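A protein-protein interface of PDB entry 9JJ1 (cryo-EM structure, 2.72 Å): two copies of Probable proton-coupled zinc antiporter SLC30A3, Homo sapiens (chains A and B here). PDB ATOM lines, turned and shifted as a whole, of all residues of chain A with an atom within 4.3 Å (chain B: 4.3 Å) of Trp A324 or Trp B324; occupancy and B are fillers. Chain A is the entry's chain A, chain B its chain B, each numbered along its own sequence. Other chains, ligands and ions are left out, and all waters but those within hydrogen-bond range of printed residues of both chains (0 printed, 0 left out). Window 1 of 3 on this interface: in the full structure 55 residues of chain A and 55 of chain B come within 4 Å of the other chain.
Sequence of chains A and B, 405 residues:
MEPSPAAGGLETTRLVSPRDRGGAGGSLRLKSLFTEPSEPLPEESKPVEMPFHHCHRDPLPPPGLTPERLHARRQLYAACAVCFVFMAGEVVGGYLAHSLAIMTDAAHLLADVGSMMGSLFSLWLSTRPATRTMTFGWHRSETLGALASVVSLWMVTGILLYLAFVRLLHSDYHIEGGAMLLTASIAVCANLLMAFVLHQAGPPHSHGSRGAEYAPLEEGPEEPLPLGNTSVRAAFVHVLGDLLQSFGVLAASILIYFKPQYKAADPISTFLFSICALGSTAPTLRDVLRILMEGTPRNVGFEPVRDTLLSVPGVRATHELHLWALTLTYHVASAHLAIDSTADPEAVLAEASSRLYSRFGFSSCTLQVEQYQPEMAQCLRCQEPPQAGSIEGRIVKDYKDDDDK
Phe A136 touches Glu B294, and with the chains exchanged Glu A294 touches Phe B136. Phe A136 touches Trp B324, and with the chains exchanged Trp A324 touches Phe B136. Glu A294 touches its own counterpart, Glu B294. Trp B324 touches its own counterpart, Trp A324. Positions printed for both chains: 136, 294, 295, 297, 322, 323, 324, 325, 331, 332 and 334.
OE1 of Glu A294 is in hydrogen-bond range of NE1 of Trp B324 (3.4 Å). The side-chain carboxylate of Glu A294 sits close to the side-chain carboxylate of Glu B294 (2.7 Å). NE1 of Trp A324 sits at hydrogen-bond distance from OE2 of Glu B294 (3.3 Å).
The backbone carbonyl oxygen (O) of Trp B324 is in hydrogen-bond range of the backbone NH (N) of Val B332. N of His A322 lies within hydrogen-bond range of O of Ser A334, at 2.8 Å. The indole nitrogen (NE1) of Trp A324 lies close to the side-chain carboxylate (OE1) of Glu A294, at 3.4 Å. The backbone NH (N) of His B322 sits at hydrogen-bond distance from the backbone carbonyl oxygen (O) of Ser B334 (2.7 Å). OE2 of Glu B294 lies close to NE1 of Trp B324 (3.4 Å). N of Val A332 lies within hydrogen-bond range of O of Trp A324 (2.7 Å).
Of the 11 printed residues of chain A, 4 touch a printed residue of chain B. Printed residues of chain A that touch a printed residue of chain B: Phe A136, Glu A294, His A322 and Trp A324. Hydrophobic or aromatic side chains of chain B that line the printed part of chain A: Phe B136, His B322 and Trp B324.
Glu B294 touches Phe A136. CZ of Phe A136 touches CG of His B322, at 3.6 Å. Trp B324 touches Phe A136 (CE3 to CE2, 3.5 Å). Glu A294 touches Phe B136 (CG to CD2, 3.5 Å). Phe B136 touches His A322 (CZ to CG, 3.6 Å). Phe B136 touches Trp A324 (CE2 to CE3, 3.5 Å). Trp A324 touches Trp B324 (CZ2 to CZ2, 3.5 Å).
Trp A324 touches just these residues of chain B: Phe B136, Glu B294 and Trp B324. Of chain A, only Phe A136 (3.5 Å), Glu A294 (3.4 Å) and Trp A324 (3.5 Å) come within 4 Å of Trp B324. Printed residues of chain B within 4 Å of His A322: Phe B136. Of the printed residues of chain A, Phe B136 touches Glu A294 (3.5 Å), His A322 (3.6 Å) and Trp A324 (3.5 Å). His B331 touches none of the printed residues of chain A. Pro B297 touches none of the printed residues of chain A. The nearest printed residue of chain B that does not touch Trp A324 is Ser B334 (5.5 Å). The nearest printed residue of chain A that does not touch His B322 is Val A332 (6.0 Å).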
ATOM      1  N   PHE A 136     -20.664  18.890  -3.372  1.00  0.00           N
ATOM      2  CA  PHE A 136     -21.000  20.275  -3.667  1.00  0.00           C
ATOM      3  C   PHE A 136     -20.933  20.606  -5.150  1.00  0.00           C
ATOM      4  O   PHE A 136     -21.456  21.649  -5.557  1.00  0.00           O
ATOM      5  CB  PHE A 136     -20.068  21.212  -2.901  1.00  0.00           C
ATOM      6  CG  PHE A 136     -20.487  21.458  -1.485  1.00  0.00           C
ATOM      7  CD1 PHE A 136     -21.498  22.351  -1.195  1.00  0.00           C
ATOM      8  CD2 PHE A 136     -19.867  20.797  -0.444  1.00  0.00           C
ATOM      9  CE1 PHE A 136     -21.882  22.579   0.106  1.00  0.00           C
ATOM     10  CE2 PHE A 136     -20.247  21.021   0.856  1.00  0.00           C
ATOM     11  CZ  PHE A 136     -21.255  21.914   1.132  1.00  0.00           C
ATOM     12  N   GLU A 294     -12.046  28.707   4.229  1.00  0.00           N
ATOM     13  CA  GLU A 294     -13.395  28.534   4.762  1.00  0.00           C
ATOM     14  C   GLU A 294     -13.831  29.744   5.581  1.00  0.00           C
ATOM     15  O   GLU A 294     -14.451  29.614   6.637  1.00  0.00           O
ATOM     16  CB  GLU A 294     -13.500  27.252   5.589  1.00  0.00           C
ATOM     17  CG  GLU A 294     -14.754  26.452   5.333  1.00  0.00           C
ATOM     18  CD  GLU A 294     -14.692  25.655   4.053  1.00  0.00           C
ATOM     19  OE1 GLU A 294     -15.637  24.887   3.795  1.00  0.00           O
ATOM     20  OE2 GLU A 294     -13.703  25.786   3.305  1.00  0.00           O
ATOM     21  N   GLY A 295     -13.504  30.935   5.089  1.00  0.00           N
ATOM     22  CA  GLY A 295     -13.913  32.154   5.751  1.00  0.00           C
ATOM     23  C   GLY A 295     -15.250  32.668   5.254  1.00  0.00           C
ATOM     24  O   GLY A 295     -15.787  32.211   4.250  1.00  0.00           O
ATOM     25  N   PRO A 297     -17.909  34.871   3.395  1.00  0.00           N
ATOM     26  CA  PRO A 297     -17.849  35.627   2.140  1.00  0.00           C
ATOM     27  C   PRO A 297     -17.770  37.124   2.399  1.00  0.00           C
ATOM     28  O   PRO A 297     -18.288  37.634   3.393  1.00  0.00           O
ATOM     29  CB  PRO A 297     -19.154  35.247   1.429  1.00  0.00           C
ATOM     30  CG  PRO A 297     -19.992  34.569   2.458  1.00  0.00           C
ATOM     31  CD  PRO A 297     -19.052  33.949   3.421  1.00  0.00           C
ATOM     32  N   HIS A 322     -22.413  28.855  10.519  1.00  0.00           N
ATOM     33  CA  HIS A 322     -21.282  28.765   9.609  1.00  0.00           C
ATOM     34  C   HIS A 322     -21.649  29.397   8.277  1.00  0.00           C
ATOM     35  O   HIS A 322     -22.672  29.049   7.683  1.00  0.00           O
ATOM     36  CB  HIS A 322     -20.861  27.312   9.398  1.00  0.00           C
ATOM     37  CG  HIS A 322     -20.316  26.656  10.626  1.00  0.00           C
ATOM     38  ND1 HIS A 322     -19.263  27.178  11.342  1.00  0.00           N
ATOM     39  CD2 HIS A 322     -20.680  25.521  11.264  1.00  0.00           C
ATOM     40  CE1 HIS A 322     -19.001  26.392  12.370  1.00  0.00           C
ATOM     41  NE2 HIS A 322     -19.847  25.380  12.346  1.00  0.00           N
ATOM     42  N   LEU A 323     -20.816  30.325   7.818  1.00  0.00           N
ATOM     43  CA  LEU A 323     -20.977  30.958   6.520  1.00  0.00           C
ATOM     44  C   LEU A 323     -19.675  30.823   5.752  1.00  0.00           C
ATOM     45  O   LEU A 323     -18.615  31.205   6.257  1.00  0.00           O
ATOM     46  CB  LEU A 323     -21.354  32.433   6.656  1.00  0.00           C
ATOM     47  CG  LEU A 323     -22.510  32.762   7.596  1.00  0.00           C
ATOM     48  CD1 LEU A 323     -22.545  34.248   7.877  1.00  0.00           C
ATOM     49  CD2 LEU A 323     -23.821  32.302   7.000  1.00  0.00           C
ATOM     50  N   TRP A 324     -19.752  30.277   4.544  1.00  0.00           N
ATOM     51  CA  TRP A 324     -18.578  30.158   3.696  1.00  0.00           C
ATOM     52  C   TRP A 324     -19.029  30.095   2.248  1.00  0.00           C
ATOM     53  O   TRP A 324     -20.206  29.883   1.952  1.00  0.00           O
ATOM     54  CB  TRP A 324     -17.728  28.937   4.068  1.00  0.00           C
ATOM     55  CG  TRP A 324     -18.296  27.623   3.648  1.00  0.00           C
ATOM     56  CD1 TRP A 324     -17.893  26.856   2.599  1.00  0.00           C
ATOM     57  CD2 TRP A 324     -19.357  26.907   4.284  1.00  0.00           C
ATOM     58  NE1 TRP A 324     -18.641  25.710   2.535  1.00  0.00           N
ATOM     59  CE2 TRP A 324     -19.550  25.718   3.559  1.00  0.00           C
ATOM     60  CE3 TRP A 324     -20.167  27.158   5.392  1.00  0.00           C
ATOM     61  CZ2 TRP A 324     -20.515  24.784   3.907  1.00  0.00           C
ATOM     62  CZ3 TRP A 324     -21.125  26.230   5.734  1.00  0.00           C
ATOM     63  CH2 TRP A 324     -21.293  25.060   4.995  1.00  0.00           C
ATOM     64  N   ALA A 325     -18.076  30.294   1.345  1.00  0.00           N
ATOM     65  CA  ALA A 325     -18.356  30.414  -0.075  1.00  0.00           C
ATOM     66  C   ALA A 325     -17.544  29.395  -0.854  1.00  0.00           C
ATOM     67  O   ALA A 325     -16.334  29.271  -0.646  1.00  0.00           O
ATOM     68  CB  ALA A 325     -18.042  31.825  -0.572  1.00  0.00           C
ATOM     69  N   HIS A 331     -22.510  30.820  -2.291  1.00  0.00           N
ATOM     70  CA  HIS A 331     -22.421  30.960  -0.846  1.00  0.00           C
ATOM     71  C   HIS A 331     -23.224  29.864  -0.163  1.00  0.00           C
ATOM     72  O   HIS A 331     -24.326  29.523  -0.600  1.00  0.00           O
ATOM     73  CB  HIS A 331     -22.934  32.328  -0.395  1.00  0.00           C
ATOM     74  CG  HIS A 331     -22.234  33.480  -1.042  1.00  0.00           C
ATOM     75  ND1 HIS A 331     -20.899  33.445  -1.380  1.00  0.00           N
ATOM     76  CD2 HIS A 331     -22.685  34.700  -1.416  1.00  0.00           C
ATOM     77  CE1 HIS A 331     -20.557  34.595  -1.930  1.00  0.00           C
ATOM     78  NE2 HIS A 331     -21.622  35.374  -1.965  1.00  0.00           N
ATOM     79  N   VAL A 332     -22.666  29.313   0.911  1.00  0.00           N
ATOM     80  CA  VAL A 332     -23.310  28.264   1.688  1.00  0.00           C
ATOM     81  C   VAL A 332     -23.495  28.764   3.112  1.00  0.00           C
ATOM     82  O   VAL A 332     -22.710  29.575   3.611  1.00  0.00           O
ATOM     83  CB  VAL A 332     -22.493  26.955   1.672  1.00  0.00           C
ATOM     84  CG1 VAL A 332     -23.354  25.786   2.099  1.00  0.00           C
ATOM     85  CG2 VAL A 332     -21.904  26.714   0.298  1.00  0.00           C
ATOM     86  N   SER A 334     -25.037  27.496   7.219  1.00  0.00           N
ATOM     87  CA  SER A 334     -25.558  26.504   8.148  1.00  0.00           C
ATOM     88  C   SER A 334     -25.700  27.167   9.508  1.00  0.00           C
ATOM     89  O   SER A 334     -24.984  28.115   9.833  1.00  0.00           O
ATOM     90  CB  SER A 334     -24.652  25.275   8.236  1.00  0.00           C
ATOM     91  OG  SER A 334     -24.202  24.875   6.957  1.00  0.00           O
ATOM     92  N   PHE B 136     -15.400  28.526  10.968  1.00  0.00           N
ATOM     93  CA  PHE B 136     -14.948  27.164  11.211  1.00  0.00           C
ATOM     94  C   PHE B 136     -13.665  27.096  12.025  1.00  0.00           C
ATOM     95  O   PHE B 136     -13.331  26.020  12.531  1.00  0.00           O
ATOM     96  CB  PHE B 136     -14.735  26.442   9.881  1.00  0.00           C
ATOM     97  CG  PHE B 136     -15.990  25.883   9.290  1.00  0.00           C
ATOM     98  CD1 PHE B 136     -16.528  24.704   9.764  1.00  0.00           C
ATOM     99  CD2 PHE B 136     -16.631  26.535   8.254  1.00  0.00           C
ATOM    100  CE1 PHE B 136     -17.681  24.188   9.219  1.00  0.00           C
ATOM    101  CE2 PHE B 136     -17.781  26.023   7.707  1.00  0.00           C
ATOM    102  CZ  PHE B 136     -18.306  24.848   8.188  1.00  0.00           C
ATOM    103  N   GLU B 294     -13.504  20.746  -1.830  1.00  0.00           N
ATOM    104  CA  GLU B 294     -14.720  20.429  -1.083  1.00  0.00           C
ATOM    105  C   GLU B 294     -15.242  19.039  -1.433  1.00  0.00           C
ATOM    106  O   GLU B 294     -16.446  18.825  -1.577  1.00  0.00           O
ATOM    107  CB  GLU B 294     -15.797  21.489  -1.311  1.00  0.00           C
ATOM    108  CG  GLU B 294     -16.591  21.832  -0.078  1.00  0.00           C
ATOM    109  CD  GLU B 294     -15.910  22.869   0.779  1.00  0.00           C
ATOM    110  OE1 GLU B 294     -14.743  23.208   0.497  1.00  0.00           O
ATOM    111  OE2 GLU B 294     -16.546  23.350   1.735  1.00  0.00           O
ATOM    112  N   GLY B 295     -14.328  18.085  -1.569  1.00  0.00           N
ATOM    113  CA  GLY B 295     -14.708  16.718  -1.844  1.00  0.00           C
ATOM    114  C   GLY B 295     -14.910  15.903  -0.582  1.00  0.00           C
ATOM    115  O   GLY B 295     -14.567  16.320   0.520  1.00  0.00           O
ATOM    116  N   PRO B 297     -14.287  13.302   2.287  1.00  0.00           N
ATOM    117  CA  PRO B 297     -13.055  12.797   2.899  1.00  0.00           C
ATOM    118  C   PRO B 297     -12.760  11.372   2.454  1.00  0.00           C
ATOM    119  O   PRO B 297     -13.665  10.588   2.167  1.00  0.00           O
ATOM    120  CB  PRO B 297     -13.346  12.867   4.404  1.00  0.00           C
ATOM    121  CG  PRO B 297     -14.812  13.099   4.522  1.00  0.00           C
ATOM    122  CD  PRO B 297     -15.223  13.822   3.294  1.00  0.00           C
ATOM    123  N   HIS B 322     -24.136  16.528   2.283  1.00  0.00           N
ATOM    124  CA  HIS B 322     -22.832  17.096   1.981  1.00  0.00           C
ATOM    125  C   HIS B 322     -21.815  16.590   2.989  1.00  0.00           C
ATOM    126  O   HIS B 322     -22.032  16.690   4.198  1.00  0.00           O
ATOM    127  CB  HIS B 322     -22.875  18.623   2.009  1.00  0.00           C
ATOM    128  CG  HIS B 322     -23.712  19.224   0.926  1.00  0.00           C
ATOM    129  ND1 HIS B 322     -23.511  18.949  -0.408  1.00  0.00           N
ATOM    130  CD2 HIS B 322     -24.753  20.086   0.980  1.00  0.00           C
ATOM    131  CE1 HIS B 322     -24.393  19.616  -1.129  1.00  0.00           C
ATOM    132  NE2 HIS B 322     -25.158  20.314  -0.311  1.00  0.00           N
ATOM    133  N   LEU B 323     -20.710  16.046   2.487  1.00  0.00           N
ATOM    134  CA  LEU B 323     -19.603  15.599   3.318  1.00  0.00           C
ATOM    135  C   LEU B 323     -18.325  16.233   2.804  1.00  0.00           C
ATOM    136  O   LEU B 323     -18.009  16.120   1.616  1.00  0.00           O
ATOM    137  CB  LEU B 323     -19.474  14.076   3.305  1.00  0.00           C
ATOM    138  CG  LEU B 323     -20.742  13.276   3.584  1.00  0.00           C
ATOM    139  CD1 LEU B 323     -20.533  11.823   3.220  1.00  0.00           C
ATOM    140  CD2 LEU B 323     -21.138  13.410   5.038  1.00  0.00           C
ATOM    141  N   TRP B 324     -17.596  16.903   3.690  1.00  0.00           N
ATOM    142  CA  TRP B 324     -16.322  17.496   3.323  1.00  0.00           C
ATOM    143  C   TRP B 324     -15.470  17.634   4.572  1.00  0.00           C
ATOM    144  O   TRP B 324     -15.960  17.522   5.696  1.00  0.00           O
ATOM    145  CB  TRP B 324     -16.502  18.847   2.621  1.00  0.00           C
ATOM    146  CG  TRP B 324     -16.889  19.975   3.518  1.00  0.00           C
ATOM    147  CD1 TRP B 324     -16.084  20.975   3.968  1.00  0.00           C
ATOM    148  CD2 TRP B 324     -18.188  20.233   4.058  1.00  0.00           C
ATOM    149  NE1 TRP B 324     -16.795  21.836   4.762  1.00  0.00           N
ATOM    150  CE2 TRP B 324     -18.091  21.402   4.833  1.00  0.00           C
ATOM    151  CE3 TRP B 324     -19.421  19.588   3.965  1.00  0.00           C
ATOM    152  CZ2 TRP B 324     -19.179  21.936   5.510  1.00  0.00           C
ATOM    153  CZ3 TRP B 324     -20.497  20.119   4.638  1.00  0.00           C
ATOM    154  CH2 TRP B 324     -20.371  21.279   5.401  1.00  0.00           C
ATOM    155  N   ALA B 325     -14.181  17.867   4.360  1.00  0.00           N
ATOM    156  CA  ALA B 325     -13.202  17.881   5.433  1.00  0.00           C
ATOM    157  C   ALA B 325     -12.445  19.198   5.434  1.00  0.00           C
ATOM    158  O   ALA B 325     -11.972  19.645   4.385  1.00  0.00           O
ATOM    159  CB  ALA B 325     -12.222  16.716   5.288  1.00  0.00           C
ATOM    160  N   HIS B 331     -13.688  16.599   9.956  1.00  0.00           N
ATOM    161  CA  HIS B 331     -14.712  16.273   8.976  1.00  0.00           C
ATOM    162  C   HIS B 331     -16.016  16.967   9.338  1.00  0.00           C
ATOM    163  O   HIS B 331     -16.392  17.029  10.512  1.00  0.00           O
ATOM    164  CB  HIS B 331     -14.939  14.764   8.896  1.00  0.00           C
ATOM    165  CG  HIS B 331     -13.703  13.983   8.583  1.00  0.00           C
ATOM    166  ND1 HIS B 331     -12.707  14.462   7.760  1.00  0.00           N
ATOM    167  CD2 HIS B 331     -13.301  12.754   8.982  1.00  0.00           C
ATOM    168  CE1 HIS B 331     -11.746  13.562   7.666  1.00  0.00           C
ATOM    169  NE2 HIS B 331     -12.081  12.516   8.398  1.00  0.00           N
ATOM    170  N   VAL B 332     -16.704  17.483   8.323  1.00  0.00           N
ATOM    171  CA  VAL B 332     -17.984  18.156   8.495  1.00  0.00           C
ATOM    172  C   VAL B 332     -19.036  17.401   7.700  1.00  0.00           C
ATOM    173  O   VAL B 332     -18.734  16.764   6.688  1.00  0.00           O
ATOM    174  CB  VAL B 332     -17.920  19.633   8.050  1.00  0.00           C
ATOM    175  CG1 VAL B 332     -19.023  20.432   8.711  1.00  0.00           C
ATOM    176  CG2 VAL B 332     -16.565  20.227   8.371  1.00  0.00           C
ATOM    177  N   SER B 334     -23.463  17.513   6.542  1.00  0.00           N
ATOM    178  CA  SER B 334     -24.766  18.162   6.507  1.00  0.00           C
ATOM    179  C   SER B 334     -25.699  17.294   5.682  1.00  0.00           C
ATOM    180  O   SER B 334     -25.267  16.567   4.786  1.00  0.00           O
ATOM    181  CB  SER B 334     -24.681  19.574   5.926  1.00  0.00           C
ATOM    182  OG  SER B 334     -23.692  20.340   6.584  1.00  0.00           O
